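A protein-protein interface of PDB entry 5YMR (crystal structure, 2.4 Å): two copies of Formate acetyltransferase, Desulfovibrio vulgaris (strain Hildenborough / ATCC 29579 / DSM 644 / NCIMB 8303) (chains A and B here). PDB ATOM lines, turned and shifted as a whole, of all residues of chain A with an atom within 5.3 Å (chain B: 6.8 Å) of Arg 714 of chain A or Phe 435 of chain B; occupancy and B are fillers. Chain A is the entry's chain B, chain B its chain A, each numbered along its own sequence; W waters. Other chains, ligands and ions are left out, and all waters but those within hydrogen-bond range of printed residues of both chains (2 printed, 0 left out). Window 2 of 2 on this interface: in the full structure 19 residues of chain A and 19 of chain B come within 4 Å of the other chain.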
ATOM      1  N   PRO A 426     -25.304   9.473   1.464  1.00  0.00           N
ATOM      2  CA  PRO A 426     -24.211  10.250   0.849  1.00  0.00           C
ATOM      3  C   PRO A 426     -23.685  11.335   1.761  1.00  0.00           C
ATOM      4  O   PRO A 426     -22.464  11.511   1.875  1.00  0.00           O
ATOM      5  CB  PRO A 426     -24.851  10.825  -0.431  1.00  0.00           C
ATOM      6  CG  PRO A 426     -25.973   9.906  -0.742  1.00  0.00           C
ATOM      7  CD  PRO A 426     -26.521   9.485   0.630  1.00  0.00           C
ATOM      8  N   LEU A 427     -24.567  12.039   2.472  1.00  0.00           N
ATOM      9  CA  LEU A 427     -24.091  13.083   3.373  1.00  0.00           C
ATOM     10  C   LEU A 427     -23.203  12.501   4.462  1.00  0.00           C
ATOM     11  O   LEU A 427     -22.198  13.115   4.853  1.00  0.00           O
ATOM     12  CB  LEU A 427     -25.276  13.839   3.984  1.00  0.00           C
ATOM     13  CG  LEU A 427     -25.938  14.884   3.066  1.00  0.00           C
ATOM     14  CD1 LEU A 427     -27.334  15.280   3.552  1.00  0.00           C
ATOM     15  CD2 LEU A 427     -25.071  16.114   2.900  1.00  0.00           C
ATOM     16  N   SER A 430     -19.851  11.374   3.216  1.00  0.00           N
ATOM     17  CA  SER A 430     -19.073  12.573   2.917  1.00  0.00           C
ATOM     18  C   SER A 430     -18.481  13.205   4.176  1.00  0.00           C
ATOM     19  O   SER A 430     -17.530  13.990   4.071  1.00  0.00           O
ATOM     20  CB  SER A 430     -19.930  13.587   2.148  1.00  0.00           C
ATOM     21  OG  SER A 430     -20.812  14.318   2.995  1.00  0.00           O
ATOM     22  N   LYS A 431     -18.999  12.855   5.362  1.00  0.00           N
ATOM     23  CA  LYS A 431     -18.497  13.379   6.626  1.00  0.00           C
ATOM     24  C   LYS A 431     -17.724  12.326   7.419  1.00  0.00           C
ATOM     25  O   LYS A 431     -17.490  12.504   8.621  1.00  0.00           O
ATOM     26  CB  LYS A 431     -19.655  13.955   7.444  1.00  0.00           C
ATOM     27  CG  LYS A 431     -20.353  15.105   6.686  1.00  0.00           C
ATOM     28  CD  LYS A 431     -21.647  15.596   7.323  1.00  0.00           C
ATOM     29  CE  LYS A 431     -22.260  16.715   6.472  1.00  0.00           C
ATOM     30  NZ  LYS A 431     -23.599  17.198   6.959  1.00  0.00           N
ATOM     31  N   VAL A 639     -25.655  27.222   4.737  1.00  0.00           N
ATOM     32  CA  VAL A 639     -24.738  26.160   4.343  1.00  0.00           C
ATOM     33  C   VAL A 639     -23.303  26.674   4.331  1.00  0.00           C
ATOM     34  O   VAL A 639     -22.405  26.080   4.948  1.00  0.00           O
ATOM     35  CB  VAL A 639     -25.155  25.580   2.979  1.00  0.00           C
ATOM     36  CG1 VAL A 639     -24.143  24.556   2.496  1.00  0.00           C
ATOM     37  CG2 VAL A 639     -26.515  24.934   3.111  1.00  0.00           C
ATOM     38  N   HIS A 652     -19.404  19.202  12.755  1.00  0.00           N
ATOM     39  CA  HIS A 652     -20.277  19.656  11.671  1.00  0.00           C
ATOM     40  C   HIS A 652     -21.479  20.292  12.350  1.00  0.00           C
ATOM     41  O   HIS A 652     -22.317  19.602  12.952  1.00  0.00           O
ATOM     42  CB  HIS A 652     -20.675  18.502  10.750  1.00  0.00           C
ATOM     43  CG  HIS A 652     -19.500  17.766  10.179  1.00  0.00           C
ATOM     44  ND1 HIS A 652     -18.979  18.035   8.927  1.00  0.00           N
ATOM     45  CD2 HIS A 652     -18.721  16.791  10.709  1.00  0.00           C
ATOM     46  CE1 HIS A 652     -17.951  17.240   8.702  1.00  0.00           C
ATOM     47  NE2 HIS A 652     -17.770  16.476   9.768  1.00  0.00           N
ATOM     48  N   ASP A 654     -24.446  21.964  11.298  1.00  0.00           N
ATOM     49  CA  ASP A 654     -25.147  22.107  10.029  1.00  0.00           C
ATOM     50  C   ASP A 654     -26.524  22.739  10.189  1.00  0.00           C
ATOM     51  O   ASP A 654     -27.271  22.420  11.119  1.00  0.00           O
ATOM     52  CB  ASP A 654     -25.279  20.742   9.346  1.00  0.00           C
ATOM     53  CG  ASP A 654     -23.929  20.166   8.949  1.00  0.00           C
ATOM     54  OD1 ASP A 654     -23.045  20.954   8.568  1.00  0.00           O
ATOM     55  OD2 ASP A 654     -23.742  18.936   9.037  1.00  0.00           O
ATOM     56  N   TYR A 711     -27.248  21.390  -3.170  1.00  0.00           N
ATOM     57  CA  TYR A 711     -26.657  20.060  -3.125  1.00  0.00           C
ATOM     58  C   TYR A 711     -25.175  20.058  -3.458  1.00  0.00           C
ATOM     59  O   TYR A 711     -24.528  19.019  -3.313  1.00  0.00           O
ATOM     60  CB  TYR A 711     -27.403  19.125  -4.059  1.00  0.00           C
ATOM     61  CG  TYR A 711     -28.806  18.782  -3.614  1.00  0.00           C
ATOM     62  CD1 TYR A 711     -29.036  17.758  -2.694  1.00  0.00           C
ATOM     63  CD2 TYR A 711     -29.913  19.440  -4.159  1.00  0.00           C
ATOM     64  CE1 TYR A 711     -30.337  17.420  -2.314  1.00  0.00           C
ATOM     65  CE2 TYR A 711     -31.200  19.106  -3.799  1.00  0.00           C
ATOM     66  CZ  TYR A 711     -31.406  18.098  -2.878  1.00  0.00           C
ATOM     67  OH  TYR A 711     -32.684  17.777  -2.507  1.00  0.00           O
ATOM     68  N   GLY A 712     -24.622  21.183  -3.915  1.00  0.00           N
ATOM     69  CA  GLY A 712     -23.203  21.234  -4.178  1.00  0.00           C
ATOM     70  C   GLY A 712     -22.325  21.235  -2.947  1.00  0.00           C
ATOM     71  O   GLY A 712     -21.108  21.087  -3.089  1.00  0.00           O
ATOM     72  N   MET A 713     -22.899  21.409  -1.751  1.00  0.00           N
ATOM     73  CA  MET A 713     -22.125  21.411  -0.512  1.00  0.00           C
ATOM     74  C   MET A 713     -22.772  20.460   0.485  1.00  0.00           C
ATOM     75  O   MET A 713     -23.973  20.185   0.399  1.00  0.00           O
ATOM     76  CB  MET A 713     -22.016  22.817   0.093  1.00  0.00           C
ATOM     77  CG  MET A 713     -21.254  23.824  -0.750  1.00  0.00           C
ATOM     78  SD  MET A 713     -21.496  25.531  -0.194  1.00  0.00           S
ATOM     79  CE  MET A 713     -23.172  25.824  -0.730  1.00  0.00           C
ATOM     80  N   ARG A 714     -21.971  19.952   1.428  1.00  0.00           N
ATOM     81  CA  ARG A 714     -22.421  18.911   2.350  1.00  0.00           C
ATOM     82  C   ARG A 714     -22.986  19.431   3.663  1.00  0.00           C
ATOM     83  O   ARG A 714     -23.515  18.623   4.442  1.00  0.00           O
ATOM     84  CB  ARG A 714     -21.280  17.932   2.676  1.00  0.00           C
ATOM     85  CG  ARG A 714     -19.941  18.579   2.850  1.00  0.00           C
ATOM     86  CD  ARG A 714     -19.327  18.462   4.248  1.00  0.00           C
ATOM     87  NE  ARG A 714     -18.372  17.358   4.333  1.00  0.00           N
ATOM     88  CZ  ARG A 714     -17.229  17.391   5.027  1.00  0.00           C
ATOM     89  NH1 ARG A 714     -16.442  16.326   5.056  1.00  0.00           N
ATOM     90  NH2 ARG A 714     -16.835  18.507   5.636  1.00  0.00           N
ATOM     91  N   ASP A 715     -22.901  20.739   3.928  1.00  0.00           N
ATOM     92  CA  ASP A 715     -23.170  21.287   5.264  1.00  0.00           C
ATOM     93  C   ASP A 715     -24.668  21.550   5.443  1.00  0.00           C
ATOM     94  O   ASP A 715     -25.171  22.673   5.508  1.00  0.00           O
ATOM     95  CB  ASP A 715     -22.307  22.515   5.484  1.00  0.00           C
ATOM     96  CG  ASP A 715     -20.891  22.278   5.015  1.00  0.00           C
ATOM     97  OD1 ASP A 715     -20.630  22.405   3.801  1.00  0.00           O
ATOM     98  OD2 ASP A 715     -20.044  21.918   5.842  1.00  0.00           O
ATOM     99  N   ARG A 716     -25.388  20.453   5.565  1.00  0.00           N
ATOM    100  CA  ARG A 716     -26.837  20.475   5.577  1.00  0.00           C
ATOM    101  C   ARG A 716     -27.266  19.283   6.416  1.00  0.00           C
ATOM    102  O   ARG A 716     -26.574  18.262   6.459  1.00  0.00           O
ATOM    103  CB  ARG A 716     -27.370  20.383   4.138  1.00  0.00           C
ATOM    104  CG  ARG A 716     -28.738  19.787   3.989  1.00  0.00           C
ATOM    105  CD  ARG A 716     -28.980  19.260   2.564  1.00  0.00           C
ATOM    106  NE  ARG A 716     -27.733  19.295   1.811  1.00  0.00           N
ATOM    107  CZ  ARG A 716     -27.268  18.360   0.976  1.00  0.00           C
ATOM    108  NH1 ARG A 716     -27.918  17.229   0.724  1.00  0.00           N
ATOM    109  NH2 ARG A 716     -26.100  18.580   0.394  1.00  0.00           N
ATOM    110  N   THR B 361     -25.811  19.075 -12.740  1.00  0.00           N
ATOM    111  CA  THR B 361     -24.925  20.217 -12.639  1.00  0.00           C
ATOM    112  C   THR B 361     -24.065  20.075 -11.386  1.00  0.00           C
ATOM    113  O   THR B 361     -24.224  19.133 -10.610  1.00  0.00           O
ATOM    114  CB  THR B 361     -25.720  21.538 -12.610  1.00  0.00           C
ATOM    115  OG1 THR B 361     -26.501  21.642 -11.411  1.00  0.00           O
ATOM    116  CG2 THR B 361     -26.661  21.628 -13.801  1.00  0.00           C
ATOM    117  N   PRO B 362     -23.098  20.969 -11.188  1.00  0.00           N
ATOM    118  CA  PRO B 362     -22.362  20.968  -9.914  1.00  0.00           C
ATOM    119  C   PRO B 362     -23.260  21.219  -8.717  1.00  0.00           C
ATOM    120  O   PRO B 362     -22.822  20.992  -7.584  1.00  0.00           O
ATOM    121  CB  PRO B 362     -21.334  22.089 -10.097  1.00  0.00           C
ATOM    122  CG  PRO B 362     -21.174  22.194 -11.614  1.00  0.00           C
ATOM    123  CD  PRO B 362     -22.545  21.929 -12.154  1.00  0.00           C
ATOM    124  N   GLU B 363     -24.497  21.681  -8.926  1.00  0.00           N
ATOM    125  CA  GLU B 363     -25.413  21.931  -7.825  1.00  0.00           C
ATOM    126  C   GLU B 363     -26.475  20.845  -7.685  1.00  0.00           C
ATOM    127  O   GLU B 363     -27.380  20.987  -6.855  1.00  0.00           O
ATOM    128  CB  GLU B 363     -26.080  23.304  -7.978  1.00  0.00           C
ATOM    129  CG  GLU B 363     -25.093  24.460  -8.037  1.00  0.00           C
ATOM    130  CD  GLU B 363     -24.497  24.637  -9.427  1.00  0.00           C
ATOM    131  OE1 GLU B 363     -25.201  24.328 -10.414  1.00  0.00           O
ATOM    132  OE2 GLU B 363     -23.320  25.032  -9.545  1.00  0.00           O
ATOM    133  N   GLY B 364     -26.370  19.758  -8.452  1.00  0.00           N
ATOM    134  CA  GLY B 364     -27.277  18.621  -8.338  1.00  0.00           C
ATOM    135  C   GLY B 364     -28.568  18.733  -9.119  1.00  0.00           C
ATOM    136  O   GLY B 364     -29.401  17.821  -9.041  1.00  0.00           O
ATOM    137  N   VAL B 425     -21.282   9.179  -7.515  1.00  0.00           N
ATOM    138  CA  VAL B 425     -21.218  10.340  -6.633  1.00  0.00           C
ATOM    139  C   VAL B 425     -21.036   9.961  -5.166  1.00  0.00           C
ATOM    140  O   VAL B 425     -20.217  10.597  -4.485  1.00  0.00           O
ATOM    141  CB  VAL B 425     -22.429  11.260  -6.863  1.00  0.00           C
ATOM    142  CG1 VAL B 425     -22.454  12.347  -5.748  1.00  0.00           C
ATOM    143  CG2 VAL B 425     -22.324  11.884  -8.222  1.00  0.00           C
ATOM    144  N   PRO B 426     -21.778   9.009  -4.605  1.00  0.00           N
ATOM    145  CA  PRO B 426     -21.520   8.669  -3.200  1.00  0.00           C
ATOM    146  C   PRO B 426     -20.122   8.116  -2.997  1.00  0.00           C
ATOM    147  O   PRO B 426     -19.433   8.490  -2.039  1.00  0.00           O
ATOM    148  CB  PRO B 426     -22.623   7.652  -2.882  1.00  0.00           C
ATOM    149  CG  PRO B 426     -23.748   7.970  -3.924  1.00  0.00           C
ATOM    150  CD  PRO B 426     -22.986   8.353  -5.149  1.00  0.00           C
ATOM    151  N   VAL B 429     -17.564  11.371  -2.954  1.00  0.00           N
ATOM    152  CA  VAL B 429     -17.523  12.172  -1.733  1.00  0.00           C
ATOM    153  C   VAL B 429     -17.037  11.328  -0.563  1.00  0.00           C
ATOM    154  O   VAL B 429     -16.397  11.849   0.358  1.00  0.00           O
ATOM    155  CB  VAL B 429     -18.880  12.828  -1.443  1.00  0.00           C
ATOM    156  CG1 VAL B 429     -19.311  13.663  -2.661  1.00  0.00           C
ATOM    157  CG2 VAL B 429     -19.925  11.778  -1.037  1.00  0.00           C
ATOM    158  N   ALA B 433     -14.254  13.865  -2.057  1.00  0.00           N
ATOM    159  CA  ALA B 433     -14.699  14.881  -2.998  1.00  0.00           C
ATOM    160  C   ALA B 433     -15.815  15.715  -2.374  1.00  0.00           C
ATOM    161  O   ALA B 433     -16.704  15.186  -1.706  1.00  0.00           O
ATOM    162  CB  ALA B 433     -15.158  14.241  -4.310  1.00  0.00           C
ATOM    163  N   THR B 434     -15.739  17.033  -2.555  1.00  0.00           N
ATOM    164  CA  THR B 434     -16.909  17.853  -2.295  1.00  0.00           C
ATOM    165  C   THR B 434     -18.027  17.393  -3.215  1.00  0.00           C
ATOM    166  O   THR B 434     -17.787  16.749  -4.239  1.00  0.00           O
ATOM    167  CB  THR B 434     -16.627  19.330  -2.556  1.00  0.00           C
ATOM    168  OG1 THR B 434     -16.448  19.529  -3.968  1.00  0.00           O
ATOM    169  CG2 THR B 434     -15.414  19.830  -1.789  1.00  0.00           C
ATOM    170  N   PHE B 435     -19.267  17.724  -2.847  1.00  0.00           N
ATOM    171  CA  PHE B 435     -20.381  17.307  -3.687  1.00  0.00           C
ATOM    172  C   PHE B 435     -20.324  17.984  -5.041  1.00  0.00           C
ATOM    173  O   PHE B 435     -20.587  17.346  -6.069  1.00  0.00           O
ATOM    174  CB  PHE B 435     -21.713  17.570  -2.996  1.00  0.00           C
ATOM    175  CG  PHE B 435     -22.143  16.440  -2.111  1.00  0.00           C
ATOM    176  CD1 PHE B 435     -22.822  15.351  -2.640  1.00  0.00           C
ATOM    177  CD2 PHE B 435     -21.822  16.445  -0.770  1.00  0.00           C
ATOM    178  CE1 PHE B 435     -23.194  14.302  -1.841  1.00  0.00           C
ATOM    179  CE2 PHE B 435     -22.198  15.391   0.044  1.00  0.00           C
ATOM    180  CZ  PHE B 435     -22.885  14.322  -0.486  1.00  0.00           C
ATOM    181  N   ALA B 436     -19.934  19.255  -5.076  1.00  0.00           N
ATOM    182  CA  ALA B 436     -19.828  19.940  -6.359  1.00  0.00           C
ATOM    183  C   ALA B 436     -18.832  19.232  -7.283  1.00  0.00           C
ATOM    184  O   ALA B 436     -19.124  19.014  -8.460  1.00  0.00           O
ATOM    185  CB  ALA B 436     -19.453  21.404  -6.135  1.00  0.00           C
ATOM    186  N   GLU B 437     -17.650  18.862  -6.768  1.00  0.00           N
ATOM    187  CA  GLU B 437     -16.663  18.159  -7.595  1.00  0.00           C
ATOM    188  C   GLU B 437     -17.211  16.813  -8.070  1.00  0.00           C
ATOM    189  O   GLU B 437     -17.044  16.445  -9.237  1.00  0.00           O
ATOM    190  CB  GLU B 437     -15.323  17.977  -6.840  1.00  0.00           C
ATOM    191  CG  GLU B 437     -14.618  19.307  -6.443  1.00  0.00           C
ATOM    192  CD  GLU B 437     -13.316  19.139  -5.610  1.00  0.00           C
ATOM    193  OE1 GLU B 437     -12.424  20.005  -5.712  1.00  0.00           O
ATOM    194  OE2 GLU B 437     -13.191  18.181  -4.815  1.00  0.00           O
ATOM    195  N   ALA B 438     -17.821  16.040  -7.168  1.00  0.00           N
ATOM    196  CA  ALA B 438     -18.386  14.744  -7.552  1.00  0.00           C
ATOM    197  C   ALA B 438     -19.499  14.903  -8.581  1.00  0.00           C
ATOM    198  O   ALA B 438     -19.521  14.203  -9.597  1.00  0.00           O
ATOM    199  CB  ALA B 438     -18.916  13.999  -6.327  1.00  0.00           C
ATOM    200  N   LEU B 439     -20.444  15.808  -8.326  1.00  0.00           N
ATOM    201  CA  LEU B 439     -21.565  15.988  -9.242  1.00  0.00           C
ATOM    202  C   LEU B 439     -21.100  16.417 -10.630  1.00  0.00           C
ATOM    203  O   LEU B 439     -21.782  16.140 -11.627  1.00  0.00           O
ATOM    204  CB  LEU B 439     -22.552  17.010  -8.672  1.00  0.00           C
ATOM    205  CG  LEU B 439     -23.403  16.531  -7.486  1.00  0.00           C
ATOM    206  CD1 LEU B 439     -24.046  17.691  -6.745  1.00  0.00           C
ATOM    207  CD2 LEU B 439     -24.506  15.608  -7.995  1.00  0.00           C
ATOM    208  N   ASP B 440     -19.948  17.085 -10.722  1.00  0.00           N
ATOM    209  CA  ASP B 440     -19.456  17.606 -11.988  1.00  0.00           C
ATOM    210  C   ASP B 440     -18.506  16.648 -12.693  1.00  0.00           C
ATOM    211  O   ASP B 440     -17.739  17.078 -13.551  1.00  0.00           O
ATOM    212  CB  ASP B 440     -18.751  18.941 -11.755  1.00  0.00           C
ATOM    213  CG  ASP B 440     -18.760  19.832 -12.986  1.00  0.00           C
ATOM    214  OD1 ASP B 440     -19.631  19.621 -13.858  1.00  0.00           O
ATOM    215  OD2 ASP B 440     -17.908  20.757 -13.070  1.00  0.00           O
HETATM  216  O   HOH W   1     -19.225  19.102   0.077  1.00  0.00           O
HETATM  217  O   HOH W   2     -28.480  23.026  -5.203  1.00  0.00           O
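The backbone carbonyl oxygen (O) of Gly 712 of chain A lies within hydrogen-bond range of the backbone NH (N) of Ala 436 of chain B.
The backbone carbonyl oxygen (O) of Pro 426 of chain A lies close to the side-chain hydroxyl (OG) of Ser 430 of chain A.
The side-chain hydroxyl (OG) of Ser 430 of chain A is in hydrogen-bond range of the backbone carbonyl oxygen (O) of Leu 427 of chain A, at 2.6 Å.
The guanidinium group (NH1) of Arg 714 of chain A lies within hydrogen-bond range of the backbone carbonyl oxygen (O) of Ser 430 of chain A, at 2.8 Å.
NZ of Lys 431 of chain A lies within hydrogen-bond range of O of Arg 714 of chain A (2.9 Å).
The side-chain carboxylate (OE1) of Glu 363 of chain B lies within hydrogen-bond range of the side-chain hydroxyl (OG1) of Thr 361 of chain B (3.1 Å).
Pro 426 of chain A touches Val 429 of chain B.
O of Pro 426 of chain A touches CZ of Phe 435 of chain B (3.7 Å).
Ser 430 of chain A touches Val 429 of chain B.
Ser 430 of chain A touches Phe 435 of chain B.
CB of Tyr 711 of chain A touches O of Glu 363 of chain B, 3.4 Å away.
Tyr 711 of chain A touches Phe 435 of chain B.
Leu 439 of chain B touches Tyr 711 of chain A.
CA of Gly 712 of chain A touches O of Pro 362 of chain B, 3.4 Å away.
Phe 435 of chain B touches Gly 712 of chain A.
CE2 of Phe 435 of chain B touches CB of Arg 714 of chain A, at 3.8 Å.
Printed residues of chain B within 4 Å of Pro 426 of chain A: Val 429 (3.9 Å) and Phe 435 (3.7 Å).
Of the printed residues of chain B, Gly 712 of chain A touches Pro 362 (3.4 Å), Phe 435 (3.6 Å) and Ala 436 (2.9 Å).
Arg 714 of chain A touches just one residue of chain B: Phe 435 (3.8 Å).
Of the printed residues of chain A, Glu 363 of chain B touches Tyr 711.
Printed residues of chain A within 4 Å of Val 429 of chain B: Pro 426 and Ser 430.
Thr 434 of chain B touches none of the printed residues of chain A.
Of chain A, only Pro 426, Ser 430, Tyr 711, Gly 712 and Arg 714 come within 4 Å of Phe 435 of chain B.
Of the printed residues of chain A, Ala 436 of chain B touches Gly 712 (2.9 Å).
Asp 440 of chain B touches none of the printed residues of chain A.
Hydrophobic or aromatic side chains of chain B within 4 Å of the printed part of chain A: Val 429, Phe 435, Ala 436 and Leu 439.
Among the printed residues, no Asp or Glu carboxylate lies within 4 Å of a Lys or Arg side-chain nitrogen of the other chain.
1 position is printed for both chains.
Water W2 lies within hydrogen-bond range of the backbone carbonyl oxygen of Glu 363 of chain B (2.8 Å) and the backbone NH of Tyr 711 of chain A (2.9 Å).
Water W1 bridges N of Arg 714 of chain A and N of Phe 435 of chain B.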
